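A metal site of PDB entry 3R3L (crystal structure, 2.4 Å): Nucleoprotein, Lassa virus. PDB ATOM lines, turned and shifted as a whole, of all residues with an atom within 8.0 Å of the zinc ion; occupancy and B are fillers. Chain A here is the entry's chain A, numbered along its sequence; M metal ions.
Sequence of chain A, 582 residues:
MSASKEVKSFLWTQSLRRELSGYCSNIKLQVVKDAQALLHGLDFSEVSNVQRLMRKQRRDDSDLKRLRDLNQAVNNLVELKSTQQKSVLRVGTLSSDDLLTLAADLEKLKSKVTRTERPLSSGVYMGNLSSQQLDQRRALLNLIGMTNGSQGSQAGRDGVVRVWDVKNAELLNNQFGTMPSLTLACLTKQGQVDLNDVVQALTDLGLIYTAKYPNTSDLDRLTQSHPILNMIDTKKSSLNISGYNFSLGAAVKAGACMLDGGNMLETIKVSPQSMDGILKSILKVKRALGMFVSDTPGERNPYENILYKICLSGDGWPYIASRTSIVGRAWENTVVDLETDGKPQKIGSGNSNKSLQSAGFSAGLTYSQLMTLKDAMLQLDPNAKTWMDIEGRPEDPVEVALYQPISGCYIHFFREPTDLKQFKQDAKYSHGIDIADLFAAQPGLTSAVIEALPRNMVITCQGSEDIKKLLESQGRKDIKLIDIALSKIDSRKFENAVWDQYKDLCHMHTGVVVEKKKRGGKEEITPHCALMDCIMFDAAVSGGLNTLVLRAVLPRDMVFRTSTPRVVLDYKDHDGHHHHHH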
ATOM      1  N   GLU A 391     -13.177  25.671  14.519  1.00  0.00           N
ATOM      2  CA  GLU A 391     -13.953  24.730  15.323  1.00  0.00           C
ATOM      3  C   GLU A 391     -15.390  25.208  15.375  1.00  0.00           C
ATOM      4  O   GLU A 391     -15.657  26.405  15.351  1.00  0.00           O
ATOM      5  CB  GLU A 391     -13.360  24.575  16.738  1.00  0.00           C
ATOM      6  CG  GLU A 391     -12.036  23.820  16.789  1.00  0.00           C
ATOM      7  CD  GLU A 391     -12.095  22.426  16.181  1.00  0.00           C
ATOM      8  OE1 GLU A 391     -13.100  21.714  16.381  1.00  0.00           O
ATOM      9  OE2 GLU A 391     -11.118  22.023  15.510  1.00  0.00           O
ATOM     10  N   GLU A 399     -14.389  28.875  17.252  1.00  0.00           N
ATOM     11  CA  GLU A 399     -12.963  29.144  17.314  1.00  0.00           C
ATOM     12  C   GLU A 399     -12.387  29.261  15.914  1.00  0.00           C
ATOM     13  O   GLU A 399     -12.631  28.399  15.063  1.00  0.00           O
ATOM     14  CB  GLU A 399     -12.239  28.045  18.109  1.00  0.00           C
ATOM     15  CG  GLU A 399     -10.774  28.352  18.389  1.00  0.00           C
ATOM     16  CD  GLU A 399     -10.106  27.262  19.215  1.00  0.00           C
ATOM     17  OE1 GLU A 399     -10.143  26.088  18.784  1.00  0.00           O
ATOM     18  OE2 GLU A 399      -9.540  27.584  20.265  1.00  0.00           O
ATOM     19  N   VAL A 400     -11.625  30.327  15.687  1.00  0.00           N
ATOM     20  CA  VAL A 400     -11.023  30.604  14.375  1.00  0.00           C
ATOM     21  C   VAL A 400      -9.546  30.908  14.547  1.00  0.00           C
ATOM     22  O   VAL A 400      -9.156  31.642  15.450  1.00  0.00           O
ATOM     23  CB  VAL A 400     -11.717  31.821  13.674  1.00  0.00           C
ATOM     24  CG1 VAL A 400     -11.107  32.082  12.314  1.00  0.00           C
ATOM     25  CG2 VAL A 400     -13.223  31.601  13.550  1.00  0.00           C
ATOM     26  N   ALA A 401      -8.718  30.333  13.673  1.00  0.00           N
ATOM     27  CA  ALA A 401      -7.282  30.592  13.709  1.00  0.00           C
ATOM     28  C   ALA A 401      -6.622  30.594  12.330  1.00  0.00           C
ATOM     29  O   ALA A 401      -6.913  29.744  11.489  1.00  0.00           O
ATOM     30  CB  ALA A 401      -6.591  29.598  14.621  1.00  0.00           C
ATOM     31  N   HIS A 412      -5.926  34.498  16.409  1.00  0.00           N
ATOM     32  CA  HIS A 412      -6.610  33.549  17.277  1.00  0.00           C
ATOM     33  C   HIS A 412      -7.707  34.226  18.082  1.00  0.00           C
ATOM     34  O   HIS A 412      -7.432  35.083  18.936  1.00  0.00           O
ATOM     35  CB  HIS A 412      -5.583  32.859  18.202  1.00  0.00           C
ATOM     36  CG  HIS A 412      -6.161  31.753  19.036  1.00  0.00           C
ATOM     37  ND1 HIS A 412      -5.724  31.501  20.319  1.00  0.00           N
ATOM     38  CD2 HIS A 412      -7.118  30.838  18.770  1.00  0.00           C
ATOM     39  CE1 HIS A 412      -6.393  30.468  20.813  1.00  0.00           C
ATOM     40  NE2 HIS A 412      -7.249  30.058  19.894  1.00  0.00           N
ATOM     41  N   PHE A 413      -8.957  33.848  17.802  1.00  0.00           N
ATOM     42  CA  PHE A 413     -10.110  34.452  18.473  1.00  0.00           C
ATOM     43  C   PHE A 413     -11.301  33.496  18.596  1.00  0.00           C
ATOM     44  O   PHE A 413     -11.346  32.447  17.944  1.00  0.00           O
ATOM     45  CB  PHE A 413     -10.540  35.761  17.777  1.00  0.00           C
ATOM     46  CG  PHE A 413     -11.045  35.564  16.372  1.00  0.00           C
ATOM     47  CD1 PHE A 413     -12.397  35.362  16.121  1.00  0.00           C
ATOM     48  CD2 PHE A 413     -10.164  35.617  15.294  1.00  0.00           C
ATOM     49  CE1 PHE A 413     -12.863  35.181  14.829  1.00  0.00           C
ATOM     50  CE2 PHE A 413     -10.624  35.443  13.990  1.00  0.00           C
ATOM     51  CZ  PHE A 413     -11.985  35.238  13.760  1.00  0.00           C
ATOM     52  N   PHE A 414     -12.270  33.869  19.420  1.00  0.00           N
ATOM     53  CA  PHE A 414     -13.437  33.032  19.703  1.00  0.00           C
ATOM     54  C   PHE A 414     -14.752  33.721  19.370  1.00  0.00           C
ATOM     55  O   PHE A 414     -14.797  34.949  19.265  1.00  0.00           O
ATOM     56  CB  PHE A 414     -13.414  32.582  21.166  1.00  0.00           C
ATOM     57  CG  PHE A 414     -12.104  31.965  21.595  1.00  0.00           C
ATOM     58  CD1 PHE A 414     -11.864  30.606  21.384  1.00  0.00           C
ATOM     59  CD2 PHE A 414     -11.114  32.731  22.194  1.00  0.00           C
ATOM     60  CE1 PHE A 414     -10.661  30.036  21.763  1.00  0.00           C
ATOM     61  CE2 PHE A 414      -9.905  32.164  22.586  1.00  0.00           C
ATOM     62  CZ  PHE A 414      -9.687  30.809  22.376  1.00  0.00           C
ATOM     63  N   HIS A 431     -14.057  19.997  20.246  1.00  0.00           N
ATOM     64  CA  HIS A 431     -13.306  21.066  20.930  1.00  0.00           C
ATOM     65  C   HIS A 431     -13.344  21.070  22.460  1.00  0.00           C
ATOM     66  O   HIS A 431     -12.453  21.642  23.091  1.00  0.00           O
ATOM     67  CB  HIS A 431     -13.662  22.447  20.375  1.00  0.00           C
ATOM     68  CG  HIS A 431     -15.130  22.690  20.194  1.00  0.00           C
ATOM     69  ND1 HIS A 431     -16.022  22.707  21.253  1.00  0.00           N
ATOM     70  CD2 HIS A 431     -15.861  22.942  19.087  1.00  0.00           C
ATOM     71  CE1 HIS A 431     -17.230  22.957  20.798  1.00  0.00           C
ATOM     72  NE2 HIS A 431     -17.170  23.099  19.486  1.00  0.00           N
ATOM     73  N   ILE A 433     -15.107  22.753  24.397  1.00  0.00           N
ATOM     74  CA  ILE A 433     -15.235  24.122  24.880  1.00  0.00           C
ATOM     75  C   ILE A 433     -16.529  24.280  25.674  1.00  0.00           C
ATOM     76  O   ILE A 433     -17.601  23.888  25.208  1.00  0.00           O
ATOM     77  CB  ILE A 433     -15.178  25.163  23.730  1.00  0.00           C
ATOM     78  CG1 ILE A 433     -13.771  25.182  23.099  1.00  0.00           C
ATOM     79  CG2 ILE A 433     -15.545  26.540  24.238  1.00  0.00           C
ATOM     80  CD1 ILE A 433     -13.649  26.036  21.829  1.00  0.00           C
ATOM     81  N   TRP A 499       1.252  20.538  21.362  1.00  0.00           N
ATOM     82  CA  TRP A 499       0.659  20.878  22.650  1.00  0.00           C
ATOM     83  C   TRP A 499       1.721  21.040  23.748  1.00  0.00           C
ATOM     84  O   TRP A 499       1.570  21.886  24.626  1.00  0.00           O
ATOM     85  CB  TRP A 499      -0.380  19.848  23.071  1.00  0.00           C
ATOM     86  CG  TRP A 499      -1.705  19.988  22.392  1.00  0.00           C
ATOM     87  CD1 TRP A 499      -2.190  19.227  21.380  1.00  0.00           C
ATOM     88  CD2 TRP A 499      -2.724  20.954  22.695  1.00  0.00           C
ATOM     89  NE1 TRP A 499      -3.443  19.654  21.023  1.00  0.00           N
ATOM     90  CE2 TRP A 499      -3.792  20.719  21.806  1.00  0.00           C
ATOM     91  CE3 TRP A 499      -2.829  22.007  23.617  1.00  0.00           C
ATOM     92  CZ2 TRP A 499      -4.962  21.478  21.827  1.00  0.00           C
ATOM     93  CZ3 TRP A 499      -3.984  22.772  23.631  1.00  0.00           C
ATOM     94  CH2 TRP A 499      -5.040  22.501  22.737  1.00  0.00           C
ATOM     95  N   LYS A 503       0.928  24.850  24.466  1.00  0.00           N
ATOM     96  CA  LYS A 503      -0.272  24.797  25.321  1.00  0.00           C
ATOM     97  C   LYS A 503      -0.754  26.170  25.817  1.00  0.00           C
ATOM     98  O   LYS A 503      -1.934  26.507  25.661  1.00  0.00           O
ATOM     99  CB  LYS A 503      -0.059  23.848  26.512  1.00  0.00           C
ATOM    100  CG  LYS A 503      -1.130  23.921  27.614  1.00  0.00           C
ATOM    101  CD  LYS A 503      -2.503  23.416  27.125  1.00  0.00           C
ATOM    102  CE  LYS A 503      -3.615  23.824  28.082  1.00  0.00           C
ATOM    103  NZ  LYS A 503      -3.893  25.291  28.065  1.00  0.00           N
ATOM    104  N   LEU A 505      -0.852  28.982  24.781  1.00  0.00           N
ATOM    105  CA  LEU A 505      -1.496  29.869  23.824  1.00  0.00           C
ATOM    106  C   LEU A 505      -3.022  29.703  23.729  1.00  0.00           C
ATOM    107  O   LEU A 505      -3.693  30.564  23.161  1.00  0.00           O
ATOM    108  CB  LEU A 505      -0.848  29.742  22.432  1.00  0.00           C
ATOM    109  CG  LEU A 505       0.622  30.161  22.283  1.00  0.00           C
ATOM    110  CD1 LEU A 505       1.103  29.907  20.859  1.00  0.00           C
ATOM    111  CD2 LEU A 505       0.859  31.624  22.663  1.00  0.00           C
ATOM    112  N   CYS A 506      -3.560  28.625  24.293  1.00  0.00           N
ATOM    113  CA  CYS A 506      -5.024  28.401  24.325  1.00  0.00           C
ATOM    114  C   CYS A 506      -5.505  27.672  25.583  1.00  0.00           C
ATOM    115  O   CYS A 506      -5.112  26.538  25.854  1.00  0.00           O
ATOM    116  CB  CYS A 506      -5.490  27.670  23.070  1.00  0.00           C
ATOM    117  SG  CYS A 506      -7.286  27.717  22.816  1.00  0.00           S
ATOM    118  N   HIS A 507      -6.374  28.335  26.338  1.00  0.00           N
ATOM    119  CA  HIS A 507      -6.917  27.783  27.584  1.00  0.00           C
ATOM    120  C   HIS A 507      -8.433  27.525  27.504  1.00  0.00           C
ATOM    121  O   HIS A 507      -9.079  27.283  28.521  1.00  0.00           O
ATOM    122  CB  HIS A 507      -6.609  28.729  28.750  1.00  0.00           C
ATOM    123  CG  HIS A 507      -5.143  28.878  29.034  1.00  0.00           C
ATOM    124  ND1 HIS A 507      -4.543  28.306  30.128  1.00  0.00           N
ATOM    125  CD2 HIS A 507      -4.168  29.527  28.365  1.00  0.00           C
ATOM    126  CE1 HIS A 507      -3.251  28.601  30.125  1.00  0.00           C
ATOM    127  NE2 HIS A 507      -3.005  29.347  29.061  1.00  0.00           N
ATOM    128  N   MET A 508      -8.977  27.563  26.292  1.00  0.00           N
ATOM    129  CA  MET A 508     -10.426  27.441  26.073  1.00  0.00           C
ATOM    130  C   MET A 508     -10.940  25.997  26.110  1.00  0.00           C
ATOM    131  O   MET A 508     -12.132  25.782  26.297  1.00  0.00           O
ATOM    132  CB  MET A 508     -10.794  28.108  24.730  1.00  0.00           C
ATOM    133  CG  MET A 508     -12.283  28.390  24.525  1.00  0.00           C
ATOM    134  SD  MET A 508     -13.096  29.390  25.794  1.00  0.00           S
ATOM    135  CE  MET A 508     -12.131  30.901  25.757  1.00  0.00           C
ATOM    136  N   HIS A 509     -10.036  25.042  25.951  1.00  0.00           N
ATOM    137  CA  HIS A 509     -10.426  23.630  25.855  1.00  0.00           C
ATOM    138  C   HIS A 509     -10.240  22.897  27.183  1.00  0.00           C
ATOM    139  O   HIS A 509      -9.117  22.527  27.545  1.00  0.00           O
ATOM    140  CB  HIS A 509      -9.659  22.936  24.726  1.00  0.00           C
ATOM    141  CG  HIS A 509      -9.657  23.714  23.447  1.00  0.00           C
ATOM    142  ND1 HIS A 509     -10.680  23.641  22.526  1.00  0.00           N
ATOM    143  CD2 HIS A 509      -8.762  24.597  22.943  1.00  0.00           C
ATOM    144  CE1 HIS A 509     -10.410  24.439  21.510  1.00  0.00           C
ATOM    145  NE2 HIS A 509      -9.253  25.028  21.729  1.00  0.00           N
ATOM    146  N   PRO A 527      -8.678  17.112  22.729  1.00  0.00           N
ATOM    147  CA  PRO A 527      -9.591  18.093  22.130  1.00  0.00           C
ATOM    148  C   PRO A 527      -8.963  18.856  20.966  1.00  0.00           C
ATOM    149  O   PRO A 527      -7.763  19.146  20.995  1.00  0.00           O
ATOM    150  CB  PRO A 527      -9.888  19.050  23.285  1.00  0.00           C
ATOM    151  CG  PRO A 527      -9.671  18.258  24.510  1.00  0.00           C
ATOM    152  CD  PRO A 527      -8.559  17.303  24.195  1.00  0.00           C
ATOM    153  N   HIS A 528      -9.765  19.172  19.954  1.00  0.00           N
ATOM    154  CA  HIS A 528      -9.294  19.882  18.768  1.00  0.00           C
ATOM    155  C   HIS A 528      -9.310  21.395  18.956  1.00  0.00           C
ATOM    156  O   HIS A 528     -10.346  21.989  19.279  1.00  0.00           O
ATOM    157  CB  HIS A 528     -10.116  19.503  17.519  1.00  0.00           C
ATOM    158  CG  HIS A 528     -10.104  18.044  17.194  1.00  0.00           C
ATOM    159  ND1 HIS A 528     -11.150  17.430  16.538  1.00  0.00           N
ATOM    160  CD2 HIS A 528      -9.193  17.074  17.444  1.00  0.00           C
ATOM    161  CE1 HIS A 528     -10.878  16.148  16.390  1.00  0.00           C
ATOM    162  NE2 HIS A 528      -9.693  15.904  16.924  1.00  0.00           N
ATOM    163  N   CYS A 529      -8.142  21.988  18.743  1.00  0.00           N
ATOM    164  CA  CYS A 529      -7.944  23.422  18.832  1.00  0.00           C
ATOM    165  C   CYS A 529      -7.610  23.934  17.435  1.00  0.00           C
ATOM    166  O   CYS A 529      -6.810  23.328  16.722  1.00  0.00           O
ATOM    167  CB  CYS A 529      -6.796  23.729  19.795  1.00  0.00           C
ATOM    168  SG  CYS A 529      -6.323  25.466  19.963  1.00  0.00           S
ATOM    169  N   ALA A 530      -8.231  25.046  17.056  1.00  0.00           N
ATOM    170  CA  ALA A 530      -8.050  25.625  15.719  1.00  0.00           C
ATOM    171  C   ALA A 530      -6.610  26.028  15.461  1.00  0.00           C
ATOM    172  O   ALA A 530      -6.056  25.752  14.396  1.00  0.00           O
ATOM    173  CB  ALA A 530      -8.983  26.805  15.519  1.00  0.00           C
ATOM    174  N   LEU A 531      -6.008  26.694  16.442  1.00  0.00           N
ATOM    175  CA  LEU A 531      -4.632  27.175  16.368  1.00  0.00           C
ATOM    176  C   LEU A 531      -3.627  26.027  16.404  1.00  0.00           C
ATOM    177  O   LEU A 531      -2.679  26.010  15.620  1.00  0.00           O
ATOM    178  CB  LEU A 531      -4.349  28.166  17.496  1.00  0.00           C
ATOM    179  CG  LEU A 531      -2.916  28.653  17.719  1.00  0.00           C
ATOM    180  CD1 LEU A 531      -2.421  29.488  16.541  1.00  0.00           C
ATOM    181  CD2 LEU A 531      -2.821  29.437  19.031  1.00  0.00           C
ATOM    182  N   MET A 532      -3.846  25.068  17.306  1.00  0.00           N
ATOM    183  CA  MET A 532      -2.938  23.919  17.417  1.00  0.00           C
ATOM    184  C   MET A 532      -3.037  23.004  16.198  1.00  0.00           C
ATOM    185  O   MET A 532      -2.059  22.353  15.827  1.00  0.00           O
ATOM    186  CB  MET A 532      -3.166  23.146  18.716  1.00  0.00           C
ATOM    187  CG  MET A 532      -3.084  23.985  19.990  1.00  0.00           C
ATOM    188  SD  MET A 532      -1.527  24.851  20.246  1.00  0.00           S
ATOM    189  CE  MET A 532      -2.088  26.239  21.231  1.00  0.00           C
ATOM    190  N   ASP A 533      -4.219  22.976  15.573  1.00  0.00           N
ATOM    191  CA  ASP A 533      -4.400  22.281  14.295  1.00  0.00           C
ATOM    192  C   ASP A 533      -3.578  22.932  13.195  1.00  0.00           C
ATOM    193  O   ASP A 533      -2.870  22.252  12.461  1.00  0.00           O
ATOM    194  CB  ASP A 533      -5.878  22.237  13.898  1.00  0.00           C
ATOM    195  CG  ASP A 533      -6.615  21.061  14.509  1.00  0.00           C
ATOM    196  OD1 ASP A 533      -5.966  20.122  15.018  1.00  0.00           O
ATOM    197  OD2 ASP A 533      -7.873  21.066  14.471  1.00  0.00           O
HETATM  198 ZN    ZN M   1      -8.010  26.544  21.071  1.00  0.00          ZN
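The zinc ion is bound by the side-chain carboxylate (OE2) of Glu 399 (2.0 Å), a ring nitrogen (NE2) of His 509 (2.1 Å), the side-chain sulfur (SG) of Cys 506 (2.2 Å) and the side-chain sulfur (SG) of Cys 529 (2.3 Å).
His 412 touches the zinc ion (NE2 to ZN, 3.8 Å).
The side-chain amino group (NZ) of Lys 503 sits at hydrogen-bond distance from the backbone carbonyl oxygen (O) of Cys 506 (2.8 Å). NE2 of His 412 sits close to OE2 of Glu 399 (3.4 Å). A ring nitrogen (ND1) of His 509 sits at hydrogen-bond distance from the backbone carbonyl oxygen of His 431 (2.7 Å). O of Glu 399 lies within hydrogen-bond range of N of Glu 391, 2.8 Å away. The side-chain sulfur (SG) of Cys 529 lies close to the backbone NH (N) of Leu 531 (3.7 Å). SG of Cys 506 lies close to NE2 of His 412, 3.7 Å away. The backbone NH of Ala 530 is in hydrogen-bond range of the side-chain carboxylate of Glu 399 (2.8 Å). N of Met 532 lies close to SG of Cys 529 (3.7 Å).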
